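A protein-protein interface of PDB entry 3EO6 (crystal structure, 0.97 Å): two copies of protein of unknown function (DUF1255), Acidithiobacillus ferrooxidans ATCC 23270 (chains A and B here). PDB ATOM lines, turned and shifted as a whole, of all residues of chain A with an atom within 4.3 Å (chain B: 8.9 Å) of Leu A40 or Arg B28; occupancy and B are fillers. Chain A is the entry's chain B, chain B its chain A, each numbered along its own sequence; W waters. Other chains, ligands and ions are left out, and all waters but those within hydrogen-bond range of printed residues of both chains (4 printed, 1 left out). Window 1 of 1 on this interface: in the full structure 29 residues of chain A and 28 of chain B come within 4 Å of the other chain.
The side-chain hydroxyl (OG) of Ser B17 lies within hydrogen-bond range of the side-chain carboxylate (OD1) of Asp A101, 2.6 Å away. The guanidinium group (NH2) of Arg B28 lies within salt-bridge range of the side-chain carboxylate (OD1) of Asp A101 (2.9 Å). The side-chain carboxylate of Asp A101 lies close to the backbone carbonyl oxygen of Lys B15.
O of Arg A28 lies within hydrogen-bond range of N of Leu A40 (2.8 Å). The backbone carbonyl oxygen (O) of Lys B15 is in hydrogen-bond range of the guanidinium group (NH1) of Arg B28 (3.2 Å). The backbone carbonyl oxygen (O) of His A38 sits at hydrogen-bond distance from the backbone NH (N) of Val A30 (2.9 Å). The backbone carbonyl oxygen of Gly B14 lies within hydrogen-bond range of the guanidinium group of Arg B28. The backbone NH (N) of Leu B40 is in hydrogen-bond range of the backbone carbonyl oxygen (O) of Arg B28, 2.8 Å away. The backbone carbonyl oxygen (O) of Ser B26 lies within hydrogen-bond range of the backbone NH (N) of Leu B42 (2.9 Å).
Ser A26 touches Leu B42. Leu B40 touches Arg A28. Val A30 touches Leu B13. Leu A40 touches Arg B28. Leu A61 touches Lys B15 (O to CD, 3.8 Å). Asp A101 touches Ser B16 (OD2 to CA, 3.5 Å).
Of the printed residues of chain B, Ser A26 touches Leu B42 (3.5 Å). Of the printed residues of chain B, Arg A28 touches Leu B40 (3.4 Å). Printed residues of chain B within 4 Å of Leu A40: Arg B28. Printed residues of chain A within 4 Å of Ser B16: Asp A101 (3.5 Å). Arg B18 touches none of the printed residues of chain A. Of the printed residues of chain A, Arg B28 touches Leu A40 and Asp A101. Printed residues of chain A within 4 Å of Leu B40: Arg A28. Of the printed residues of chain A, Leu B42 touches Ser A26 (3.5 Å). The nearest printed residue of chain B that does not touch Leu A40 is Leu B13 (4.2 Å). The nearest printed residue of chain B that does not touch Ser A26 is Ser B26 (4.3 Å).
Of the 24 printed residues of chain B, 7 touch a printed residue of chain A. Printed residues of chain B that touch a printed residue of chain A: Leu B13, Lys B15, Ser B16, Ser B17, Arg B28, Leu B40 and Leu B42. Hydrophobic or aromatic side chains of chain A that line the printed part of chain B: Val A30, Leu A40 and Leu A61. Along chain A the printed residues that touch a printed residue of chain B span positions 26 to 101.
Arg A28 touches Leu B40, and with the chains exchanged Leu A40 touches Arg B28. Of the 9 pairs that touch across the chains among the printed residues, 2 have their exchanged pair printed and touching as well.
Water W3 lies within hydrogen-bond range of the backbone carbonyl oxygen of Leu A40 (2.8 Å) and the guanidinium group of Arg B28 (2.9 Å). Water W1 bridges the guanidinium group (NE) of Arg B28 (2.9 Å) and the guanidinium group (NE) of Arg A28 (2.9 Å). Water W4 lies within hydrogen-bond range of the backbone carbonyl oxygen (O) of Leu B40 (2.9 Å) and the guanidinium group (NH2) of Arg A28 (3.0 Å). Water W2 bridges O of Leu A61 (2.9 Å) and NZ of Lys B15 (3.0 Å).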
ATOM      1  N   SER A  26      20.209   5.115   4.651  1.00  0.00           N
ATOM      2  CA  SER A  26      19.898   5.368   3.254  1.00  0.00           C
ATOM      3  C   SER A  26      18.422   5.157   3.055  1.00  0.00           C
ATOM      4  O   SER A  26      17.817   4.285   3.663  1.00  0.00           O
ATOM      5  CB  SER A  26      20.736   4.487   2.335  1.00  0.00           C
ATOM      6  OG  SER A  26      20.625   3.122   2.626  1.00  0.00           O
ATOM      7  N   GLU A  27      17.872   5.903   2.128  1.00  0.00           N
ATOM      8  CA  GLU A  27      16.504   5.698   1.817  1.00  0.00           C
ATOM      9  C   GLU A  27      16.195   6.101   0.428  1.00  0.00           C
ATOM     10  O   GLU A  27      16.900   6.913  -0.186  1.00  0.00           O
ATOM     11  CB  GLU A  27      15.614   6.446   2.747  1.00  0.00           C
ATOM     12  CG  GLU A  27      15.864   7.899   2.867  1.00  0.00           C
ATOM     13  CD  GLU A  27      15.155   8.840   1.907  1.00  0.00           C
ATOM     14  OE1 GLU A  27      14.253   8.369   1.142  1.00  0.00           O
ATOM     15  OE2 GLU A  27      15.504  10.050   1.880  1.00  0.00           O
ATOM     16  N   ARG A  28      15.130   5.525  -0.082  1.00  0.00           N
ATOM     17  CA  ARG A  28      14.547   5.946  -1.357  1.00  0.00           C
ATOM     18  C   ARG A  28      13.054   6.046  -1.137  1.00  0.00           C
ATOM     19  O   ARG A  28      12.458   5.335  -0.333  1.00  0.00           O
ATOM     20  CB  ARG A  28      14.854   5.057  -2.546  1.00  0.00           C
ATOM     21  CG  ARG A  28      14.255   3.680  -2.355  1.00  0.00           C
ATOM     22  CD  ARG A  28      14.541   2.721  -3.603  1.00  0.00           C
ATOM     23  NE  ARG A  28      15.951   2.251  -3.547  1.00  0.00           N
ATOM     24  CZ  ARG A  28      16.966   2.689  -4.276  1.00  0.00           C
ATOM     25  NH1 ARG A  28      16.815   3.617  -5.245  1.00  0.00           N
ATOM     26  NH2 ARG A  28      18.163   2.148  -4.091  1.00  0.00           N
ATOM     27  N   VAL A  30       9.230   5.279  -2.159  1.00  0.00           N
ATOM     28  CA  VAL A  30       8.486   4.231  -2.818  1.00  0.00           C
ATOM     29  C   VAL A  30       6.996   4.559  -2.751  1.00  0.00           C
ATOM     30  O   VAL A  30       6.544   5.266  -1.867  1.00  0.00           O
ATOM     31  CB  VAL A  30       8.745   2.844  -2.213  1.00  0.00           C
ATOM     32  CG1 VAL A  30      10.237   2.495  -2.345  1.00  0.00           C
ATOM     33  CG2 VAL A  30       8.281   2.746  -0.750  1.00  0.00           C
ATOM     34  N   HIS A  38       6.141   6.406   0.879  1.00  0.00           N
ATOM     35  CA  HIS A  38       6.946   6.194   2.057  1.00  0.00           C
ATOM     36  C   HIS A  38       8.418   6.373   1.673  1.00  0.00           C
ATOM     37  O   HIS A  38       8.788   6.237   0.500  1.00  0.00           O
ATOM     38  CB  HIS A  38       6.781   4.760   2.639  1.00  0.00           C
ATOM     39  CG  HIS A  38       5.375   4.444   3.008  1.00  0.00           C
ATOM     40  ND1 HIS A  38       4.961   4.267   4.310  1.00  0.00           N
ATOM     41  CD2 HIS A  38       4.283   4.360   2.216  1.00  0.00           C
ATOM     42  CE1 HIS A  38       3.646   4.079   4.274  1.00  0.00           C
ATOM     43  NE2 HIS A  38       3.215   4.103   3.024  1.00  0.00           N
ATOM     44  N   SER A  39       9.249   6.592   2.686  1.00  0.00           N
ATOM     45  CA  SER A  39      10.707   6.459   2.566  1.00  0.00           C
ATOM     46  C   SER A  39      11.072   5.082   3.016  1.00  0.00           C
ATOM     47  O   SER A  39      10.896   4.702   4.179  1.00  0.00           O
ATOM     48  CB  SER A  39      11.408   7.502   3.416  1.00  0.00           C
ATOM     49  OG  SER A  39      11.079   8.791   2.995  1.00  0.00           O
ATOM     50  N   LEU A  40      11.527   4.255   2.095  1.00  0.00           N
ATOM     51  CA  LEU A  40      11.989   2.905   2.370  1.00  0.00           C
ATOM     52  C   LEU A  40      13.434   3.052   2.789  1.00  0.00           C
ATOM     53  O   LEU A  40      14.311   3.412   1.990  1.00  0.00           O
ATOM     54  CB  LEU A  40      11.832   2.032   1.135  1.00  0.00           C
ATOM     55  CG  LEU A  40      12.383   0.617   1.259  1.00  0.00           C
ATOM     56  CD1 LEU A  40      11.757  -0.130   2.455  1.00  0.00           C
ATOM     57  CD2 LEU A  40      12.198  -0.094  -0.079  1.00  0.00           C
ATOM     58  N   THR A  41      13.675   2.811   4.085  1.00  0.00           N
ATOM     59  CA  THR A  41      14.891   3.187   4.779  1.00  0.00           C
ATOM     60  C   THR A  41      15.623   1.966   5.274  1.00  0.00           C
ATOM     61  O   THR A  41      15.016   1.018   5.769  1.00  0.00           O
ATOM     62  CB  THR A  41      14.520   4.106   5.935  1.00  0.00           C
ATOM     63  OG1 THR A  41      13.698   5.178   5.500  1.00  0.00           O
ATOM     64  CG2 THR A  41      15.763   4.693   6.575  1.00  0.00           C
ATOM     65  N   LEU A  61      10.098  -3.484   8.731  1.00  0.00           N
ATOM     66  CA  LEU A  61      10.004  -4.635   7.856  1.00  0.00           C
ATOM     67  C   LEU A  61      10.917  -5.783   8.306  1.00  0.00           C
ATOM     68  O   LEU A  61      10.548  -6.947   8.144  1.00  0.00           O
ATOM     69  CB  LEU A  61      10.344  -4.253   6.409  1.00  0.00           C
ATOM     70  CG  LEU A  61       9.463  -3.136   5.840  1.00  0.00           C
ATOM     71  CD1 LEU A  61       9.960  -2.833   4.413  1.00  0.00           C
ATOM     72  CD2 LEU A  61       8.015  -3.482   5.842  1.00  0.00           C
ATOM     73  N   ASP A 101      15.318  -2.291   8.373  1.00  0.00           N
ATOM     74  CA  ASP A 101      14.599  -1.925   7.156  1.00  0.00           C
ATOM     75  C   ASP A 101      13.211  -1.457   7.576  1.00  0.00           C
ATOM     76  O   ASP A 101      12.523  -2.199   8.265  1.00  0.00           O
ATOM     77  CB  ASP A 101      14.435  -3.123   6.217  1.00  0.00           C
ATOM     78  CG  ASP A 101      15.689  -3.479   5.466  1.00  0.00           C
ATOM     79  OD1 ASP A 101      15.959  -2.767   4.472  1.00  0.00           O
ATOM     80  OD2 ASP A 101      16.382  -4.455   5.836  1.00  0.00           O
ATOM     81  N   TYR A 102      12.817  -0.263   7.153  1.00  0.00           N
ATOM     82  CA  TYR A 102      11.546   0.263   7.594  1.00  0.00           C
ATOM     83  C   TYR A 102      10.990   1.223   6.573  1.00  0.00           C
ATOM     84  O   TYR A 102      11.704   1.838   5.783  1.00  0.00           O
ATOM     85  CB  TYR A 102      11.652   0.938   8.982  1.00  0.00           C
ATOM     86  CG  TYR A 102      12.672   2.037   9.126  1.00  0.00           C
ATOM     87  CD1 TYR A 102      14.009   1.744   9.299  1.00  0.00           C
ATOM     88  CD2 TYR A 102      12.296   3.353   9.162  1.00  0.00           C
ATOM     89  CE1 TYR A 102      14.938   2.720   9.549  1.00  0.00           C
ATOM     90  CE2 TYR A 102      13.242   4.368   9.424  1.00  0.00           C
ATOM     91  CZ  TYR A 102      14.568   4.022   9.630  1.00  0.00           C
ATOM     92  OH  TYR A 102      15.543   4.946   9.925  1.00  0.00           O
ATOM     93  N   LEU A 103       9.658   1.348   6.606  1.00  0.00           N
ATOM     94  CA  LEU A 103       8.933   2.350   5.847  1.00  0.00           C
ATOM     95  C   LEU A 103       8.631   3.521   6.772  1.00  0.00           C
ATOM     96  O   LEU A 103       8.002   3.327   7.821  1.00  0.00           O
ATOM     97  CB  LEU A 103       7.641   1.780   5.327  1.00  0.00           C
ATOM     98  CG  LEU A 103       7.784   0.688   4.288  1.00  0.00           C
ATOM     99  CD1 LEU A 103       6.503  -0.133   4.187  1.00  0.00           C
ATOM    100  CD2 LEU A 103       8.139   1.279   2.934  1.00  0.00           C
ATOM    101  N   ALA B  12       6.887  -5.302  -6.429  1.00  0.00           N
ATOM    102  CA  ALA B  12       7.140  -5.709  -5.069  1.00  0.00           C
ATOM    103  C   ALA B  12       8.529  -5.317  -4.676  1.00  0.00           C
ATOM    104  O   ALA B  12       9.449  -5.278  -5.503  1.00  0.00           O
ATOM    105  CB  ALA B  12       6.987  -7.197  -4.883  1.00  0.00           C
ATOM    106  N   LEU B  13       8.707  -5.091  -3.381  1.00  0.00           N
ATOM    107  CA  LEU B  13       9.970  -4.646  -2.744  1.00  0.00           C
ATOM    108  C   LEU B  13      10.329  -5.666  -1.654  1.00  0.00           C
ATOM    109  O   LEU B  13       9.521  -5.908  -0.744  1.00  0.00           O
ATOM    110  CB  LEU B  13       9.776  -3.261  -2.110  1.00  0.00           C
ATOM    111  CG  LEU B  13       9.322  -2.200  -3.094  1.00  0.00           C
ATOM    112  CD1 LEU B  13       8.753  -0.997  -2.348  1.00  0.00           C
ATOM    113  CD2 LEU B  13      10.413  -1.817  -4.041  1.00  0.00           C
ATOM    114  N   GLY B  14      11.536  -6.227  -1.680  1.00  0.00           N
ATOM    115  CA  GLY B  14      11.981  -7.101  -0.642  1.00  0.00           C
ATOM    116  C   GLY B  14      12.117  -6.396   0.696  1.00  0.00           C
ATOM    117  O   GLY B  14      12.604  -5.271   0.744  1.00  0.00           O
ATOM    118  N   LYS B  15      11.701  -7.042   1.767  1.00  0.00           N
ATOM    119  CA  LYS B  15      11.766  -6.437   3.085  1.00  0.00           C
ATOM    120  C   LYS B  15      13.196  -6.262   3.602  1.00  0.00           C
ATOM    121  O   LYS B  15      13.490  -5.237   4.215  1.00  0.00           O
ATOM    122  CB  LYS B  15      10.999  -7.287   4.094  1.00  0.00           C
ATOM    123  CG  LYS B  15       9.492  -7.219   3.917  1.00  0.00           C
ATOM    124  CD  LYS B  15       8.801  -8.035   4.965  1.00  0.00           C
ATOM    125  CE  LYS B  15       7.314  -7.993   4.845  1.00  0.00           C
ATOM    126  NZ  LYS B  15       6.707  -8.883   5.863  1.00  0.00           N
ATOM    127  N   SER B  16      14.032  -7.277   3.415  1.00  0.00           N
ATOM    128  CA  SER B  16      15.312  -7.354   4.100  1.00  0.00           C
ATOM    129  C   SER B  16      16.475  -7.000   3.186  1.00  0.00           C
ATOM    130  O   SER B  16      16.709  -7.661   2.186  1.00  0.00           O
ATOM    131  CB  SER B  16      15.549  -8.774   4.620  1.00  0.00           C
ATOM    132  OG  SER B  16      14.600  -9.151   5.595  1.00  0.00           O
ATOM    133  N   SER B  17      17.252  -5.985   3.572  1.00  0.00           N
ATOM    134  CA  SER B  17      18.455  -5.615   2.840  1.00  0.00           C
ATOM    135  C   SER B  17      19.604  -6.530   3.212  1.00  0.00           C
ATOM    136  O   SER B  17      19.663  -7.151   4.266  1.00  0.00           O
ATOM    137  CB  SER B  17      18.842  -4.184   3.195  1.00  0.00           C
ATOM    138  OG  SER B  17      17.887  -3.242   2.753  1.00  0.00           O
ATOM    139  N   ARG B  18      20.548  -6.589   2.269  1.00  0.00           N
ATOM    140  CA  ARG B  18      21.846  -7.239   2.437  1.00  0.00           C
ATOM    141  C   ARG B  18      22.915  -6.134   2.408  1.00  0.00           C
ATOM    142  O   ARG B  18      22.969  -5.332   1.463  1.00  0.00           O
ATOM    143  CB  ARG B  18      22.022  -8.280   1.331  1.00  0.00           C
ATOM    144  CG  ARG B  18      20.891  -9.346   1.416  1.00  0.00           C
ATOM    145  CD  ARG B  18      20.943 -10.435   0.337  1.00  0.00           C
ATOM    146  NE  ARG B  18      20.748  -9.932  -1.027  1.00  0.00           N
ATOM    147  CZ  ARG B  18      19.583  -9.626  -1.589  1.00  0.00           C
ATOM    148  NH1 ARG B  18      18.436  -9.737  -0.919  1.00  0.00           N
ATOM    149  NH2 ARG B  18      19.571  -9.177  -2.843  1.00  0.00           N
ATOM    150  N   ILE B  19      23.751  -6.060   3.432  1.00  0.00           N
ATOM    151  CA  ILE B  19      24.838  -5.102   3.493  1.00  0.00           C
ATOM    152  C   ILE B  19      26.142  -5.851   3.245  1.00  0.00           C
ATOM    153  O   ILE B  19      26.343  -6.925   3.811  1.00  0.00           O
ATOM    154  CB  ILE B  19      24.849  -4.347   4.834  1.00  0.00           C
ATOM    155  CG1 ILE B  19      23.523  -3.593   5.047  1.00  0.00           C
ATOM    156  CG2 ILE B  19      26.032  -3.425   4.948  1.00  0.00           C
ATOM    157  CD1 ILE B  19      23.372  -3.055   6.452  1.00  0.00           C
ATOM    158  N   ARG B  25      27.958  -1.141   0.430  1.00  0.00           N
ATOM    159  CA  ARG B  25      26.974  -1.614  -0.509  1.00  0.00           C
ATOM    160  C   ARG B  25      25.783  -2.149   0.256  1.00  0.00           C
ATOM    161  O   ARG B  25      25.926  -2.898   1.208  1.00  0.00           O
ATOM    162  CB  ARG B  25      27.537  -2.700  -1.407  1.00  0.00           C
ATOM    163  CG  ARG B  25      26.556  -3.154  -2.480  1.00  0.00           C
ATOM    164  CD  ARG B  25      27.154  -4.049  -3.536  1.00  0.00           C
ATOM    165  NE  ARG B  25      27.707  -5.256  -2.892  1.00  0.00           N
ATOM    166  CZ  ARG B  25      28.322  -6.223  -3.528  1.00  0.00           C
ATOM    167  NH1 ARG B  25      28.448  -6.191  -4.838  1.00  0.00           N
ATOM    168  NH2 ARG B  25      28.849  -7.220  -2.853  1.00  0.00           N
ATOM    169  N   SER B  26      24.576  -1.871  -0.280  1.00  0.00           N
ATOM    170  CA  SER B  26      23.354  -2.513   0.216  1.00  0.00           C
ATOM    171  C   SER B  26      22.455  -2.868  -0.941  1.00  0.00           C
ATOM    172  O   SER B  26      22.361  -2.128  -1.907  1.00  0.00           O
ATOM    173  CB  SER B  26      22.628  -1.631   1.225  1.00  0.00           C
ATOM    174  OG  SER B  26      22.288  -0.391   0.685  1.00  0.00           O
ATOM    175  N   GLU B  27      21.795  -3.998  -0.819  1.00  0.00           N
ATOM    176  CA  GLU B  27      20.946  -4.524  -1.861  1.00  0.00           C
ATOM    177  C   GLU B  27      19.611  -4.909  -1.166  1.00  0.00           C
ATOM    178  O   GLU B  27      19.612  -5.383  -0.031  1.00  0.00           O
ATOM    179  CB  GLU B  27      21.615  -5.785  -2.454  1.00  0.00           C
ATOM    180  CG  GLU B  27      22.941  -5.524  -3.173  1.00  0.00           C
ATOM    181  CD  GLU B  27      23.648  -6.793  -3.530  1.00  0.00           C
ATOM    182  OE1 GLU B  27      23.411  -7.311  -4.659  1.00  0.00           O
ATOM    183  OE2 GLU B  27      24.406  -7.327  -2.717  1.00  0.00           O
ATOM    184  N   ARG B  28      18.481  -4.723  -1.824  1.00  0.00           N
ATOM    185  CA  ARG B  28      17.324  -5.592  -1.583  1.00  0.00           C
ATOM    186  C   ARG B  28      16.869  -6.105  -2.939  1.00  0.00           C
ATOM    187  O   ARG B  28      17.103  -5.496  -3.968  1.00  0.00           O
ATOM    188  CB  ARG B  28      16.147  -4.832  -0.891  1.00  0.00           C
ATOM    189  CG  ARG B  28      15.529  -3.749  -1.724  1.00  0.00           C
ATOM    190  CD  ARG B  28      14.441  -2.940  -1.043  1.00  0.00           C
ATOM    191  NE  ARG B  28      14.959  -1.984  -0.040  1.00  0.00           N
ATOM    192  CZ  ARG B  28      14.946  -2.145   1.284  1.00  0.00           C
ATOM    193  NH1 ARG B  28      14.443  -3.253   1.842  1.00  0.00           N
ATOM    194  NH2 ARG B  28      15.432  -1.213   2.082  1.00  0.00           N
ATOM    195  N   SER B  29      16.162  -7.206  -2.909  1.00  0.00           N
ATOM    196  CA  SER B  29      15.550  -7.757  -4.093  1.00  0.00           C
ATOM    197  C   SER B  29      14.265  -6.997  -4.400  1.00  0.00           C
ATOM    198  O   SER B  29      13.557  -6.623  -3.479  1.00  0.00           O
ATOM    199  CB  SER B  29      15.269  -9.231  -3.848  1.00  0.00           C
ATOM    200  OG  SER B  29      16.495  -9.952  -3.628  1.00  0.00           O
ATOM    201  N   VAL B  30      13.967  -6.821  -5.676  1.00  0.00           N
ATOM    202  CA  VAL B  30      12.741  -6.192  -6.122  1.00  0.00           C
ATOM    203  C   VAL B  30      12.203  -6.912  -7.346  1.00  0.00           C
ATOM    204  O   VAL B  30      12.929  -7.584  -8.085  1.00  0.00           O
ATOM    205  CB  VAL B  30      12.907  -4.676  -6.444  1.00  0.00           C
ATOM    206  CG1 VAL B  30      13.427  -3.920  -5.196  1.00  0.00           C
ATOM    207  CG2 VAL B  30      13.825  -4.467  -7.655  1.00  0.00           C
ATOM    208  N   ILE B  31      10.910  -6.788  -7.561  1.00  0.00           N
ATOM    209  CA  ILE B  31      10.274  -7.281  -8.782  1.00  0.00           C
ATOM    210  C   ILE B  31       9.684  -6.074  -9.465  1.00  0.00           C
ATOM    211  O   ILE B  31       8.894  -5.351  -8.865  1.00  0.00           O
ATOM    212  CB  ILE B  31       9.174  -8.318  -8.495  1.00  0.00           C
ATOM    213  CG1 ILE B  31       9.718  -9.470  -7.650  1.00  0.00           C
ATOM    214  CG2 ILE B  31       8.573  -8.818  -9.825  1.00  0.00           C
ATOM    215  CD1 ILE B  31       8.654 -10.353  -7.084  1.00  0.00           C
ATOM    216  N   MET B  37      13.158  -9.767 -11.949  1.00  0.00           N
ATOM    217  CA  MET B  37      13.707  -9.835 -10.648  1.00  0.00           C
ATOM    218  C   MET B  37      15.125  -9.264 -10.583  1.00  0.00           C
ATOM    219  O   MET B  37      16.031  -9.816 -11.201  1.00  0.00           O
ATOM    220  CB  MET B  37      13.738 -11.298 -10.326  1.00  0.00           C
ATOM    221  CG  MET B  37      12.378 -11.931 -10.137  1.00  0.00           C
ATOM    222  SD  MET B  37      12.571 -13.818  -9.734  1.00  0.00           S
ATOM    223  CE  MET B  37      14.262 -13.809  -8.787  1.00  0.00           C
ATOM    224  N   HIS B  38      15.336  -8.240  -9.757  1.00  0.00           N
ATOM    225  CA  HIS B  38      16.596  -7.554  -9.753  1.00  0.00           C
ATOM    226  C   HIS B  38      17.046  -7.314  -8.327  1.00  0.00           C
ATOM    227  O   HIS B  38      16.226  -7.265  -7.405  1.00  0.00           O
ATOM    228  CB  HIS B  38      16.464  -6.173 -10.422  1.00  0.00           C
ATOM    229  CG  HIS B  38      15.932  -6.210 -11.802  1.00  0.00           C
ATOM    230  ND1 HIS B  38      16.699  -5.985 -12.919  1.00  0.00           N
ATOM    231  CD2 HIS B  38      14.671  -6.481 -12.211  1.00  0.00           C
ATOM    232  CE1 HIS B  38      15.903  -6.099 -13.967  1.00  0.00           C
ATOM    233  NE2 HIS B  38      14.671  -6.402 -13.581  1.00  0.00           N
ATOM    234  N   SER B  39      18.349  -7.073  -8.159  1.00  0.00           N
ATOM    235  CA  SER B  39      18.905  -6.507  -6.935  1.00  0.00           C
ATOM    236  C   SER B  39      19.003  -5.000  -7.053  1.00  0.00           C
ATOM    237  O   SER B  39      19.785  -4.459  -7.839  1.00  0.00           O
ATOM    238  CB  SER B  39      20.297  -7.053  -6.636  1.00  0.00           C
ATOM    239  OG  SER B  39      20.245  -8.433  -6.340  1.00  0.00           O
ATOM    240  N   LEU B  40      18.204  -4.317  -6.260  1.00  0.00           N
ATOM    241  CA  LEU B  40      18.204  -2.862  -6.239  1.00  0.00           C
ATOM    242  C   LEU B  40      19.278  -2.427  -5.248  1.00  0.00           C
ATOM    243  O   LEU B  40      19.153  -2.674  -4.035  1.00  0.00           O
ATOM    244  CB  LEU B  40      16.828  -2.370  -5.828  1.00  0.00           C
ATOM    245  CG  LEU B  40      16.686  -0.867  -5.673  1.00  0.00           C
ATOM    246  CD1 LEU B  40      17.051  -0.091  -6.883  1.00  0.00           C
ATOM    247  CD2 LEU B  40      15.245  -0.556  -5.244  1.00  0.00           C
ATOM    248  N   THR B  41      20.362  -1.891  -5.786  1.00  0.00           N
ATOM    249  CA  THR B  41      21.602  -1.719  -5.085  1.00  0.00           C
ATOM    250  C   THR B  41      21.948  -0.246  -4.939  1.00  0.00           C
ATOM    251  O   THR B  41      21.760   0.519  -5.879  1.00  0.00           O
ATOM    252  CB  THR B  41      22.734  -2.434  -5.866  1.00  0.00           C
ATOM    253  OG1 THR B  41      22.317  -3.772  -6.146  1.00  0.00           O
ATOM    254  CG2 THR B  41      24.018  -2.426  -5.096  1.00  0.00           C
ATOM    255  N   LEU B  42      22.492   0.111  -3.768  1.00  0.00           N
ATOM    256  CA  LEU B  42      23.115   1.388  -3.509  1.00  0.00           C
ATOM    257  C   LEU B  42      24.586   1.105  -3.183  1.00  0.00           C
ATOM    258  O   LEU B  42      24.891   0.343  -2.269  1.00  0.00           O
ATOM    259  CB  LEU B  42      22.434   2.075  -2.340  1.00  0.00           C
ATOM    260  CG  LEU B  42      23.060   3.382  -1.937  1.00  0.00           C
ATOM    261  CD1 LEU B  42      23.047   4.434  -3.052  1.00  0.00           C
ATOM    262  CD2 LEU B  42      22.323   3.909  -0.699  1.00  0.00           C
ATOM    263  N   TYR B 102      21.459   1.302  -8.666  1.00  0.00           N
ATOM    264  CA  TYR B 102      21.353   0.506  -9.867  1.00  0.00           C
ATOM    265  C   TYR B 102      20.578  -0.747  -9.603  1.00  0.00           C
ATOM    266  O   TYR B 102      20.507  -1.223  -8.485  1.00  0.00           O
ATOM    267  CB  TYR B 102      22.759   0.183 -10.441  1.00  0.00           C
ATOM    268  CG  TYR B 102      23.727  -0.547  -9.527  1.00  0.00           C
ATOM    269  CD1 TYR B 102      24.482   0.166  -8.609  1.00  0.00           C
ATOM    270  CD2 TYR B 102      23.945  -1.886  -9.631  1.00  0.00           C
ATOM    271  CE1 TYR B 102      25.454  -0.455  -7.840  1.00  0.00           C
ATOM    272  CE2 TYR B 102      24.904  -2.528  -8.857  1.00  0.00           C
ATOM    273  CZ  TYR B 102      25.677  -1.809  -7.973  1.00  0.00           C
ATOM    274  OH  TYR B 102      26.682  -2.349  -7.227  1.00  0.00           O
ATOM    275  N   LEU B 103      20.010  -1.255 -10.685  1.00  0.00           N
ATOM    276  CA  LEU B 103      19.466  -2.572 -10.720  1.00  0.00           C
ATOM    277  C   LEU B 103      20.524  -3.507 -11.305  1.00  0.00           C
ATOM    278  O   LEU B 103      21.280  -3.157 -12.227  1.00  0.00           O
ATOM    279  CB  LEU B 103      18.202  -2.585 -11.570  1.00  0.00           C
ATOM    280  CG  LEU B 103      17.057  -1.758 -10.948  1.00  0.00           C
ATOM    281  CD1 LEU B 103      16.097  -1.189 -12.014  1.00  0.00           C
ATOM    282  CD2 LEU B 103      16.286  -2.572  -9.895  1.00  0.00           C
ATOM    283  N   LEU B 104      20.538  -4.716 -10.790  1.00  0.00           N
ATOM    284  CA  LEU B 104      21.485  -5.693 -11.261  1.00  0.00           C
ATOM    285  C   LEU B 104      20.671  -6.987 -11.344  1.00  0.00           C
ATOM    286  O   LEU B 104      20.113  -7.400 -10.322  1.00  0.00           O
ATOM    287  CB  LEU B 104      22.636  -5.795 -10.288  1.00  0.00           C
ATOM    288  CG  LEU B 104      23.789  -6.615 -10.885  1.00  0.00           C
ATOM    289  CD1 LEU B 104      24.355  -5.975 -12.176  1.00  0.00           C
ATOM    290  CD2 LEU B 104      24.893  -6.781  -9.840  1.00  0.00           C
HETATM  291  O   HOH W   1      16.085   0.270  -1.395  1.00  0.00           O
HETATM  292  O   HOH W   2       7.719  -7.537   8.353  1.00  0.00           O
HETATM  293  O   HOH W   3      16.180   1.418   1.202  1.00  0.00           O
HETATM  294  O   HOH W   4      18.667  -0.337  -2.438  1.00  0.00           O
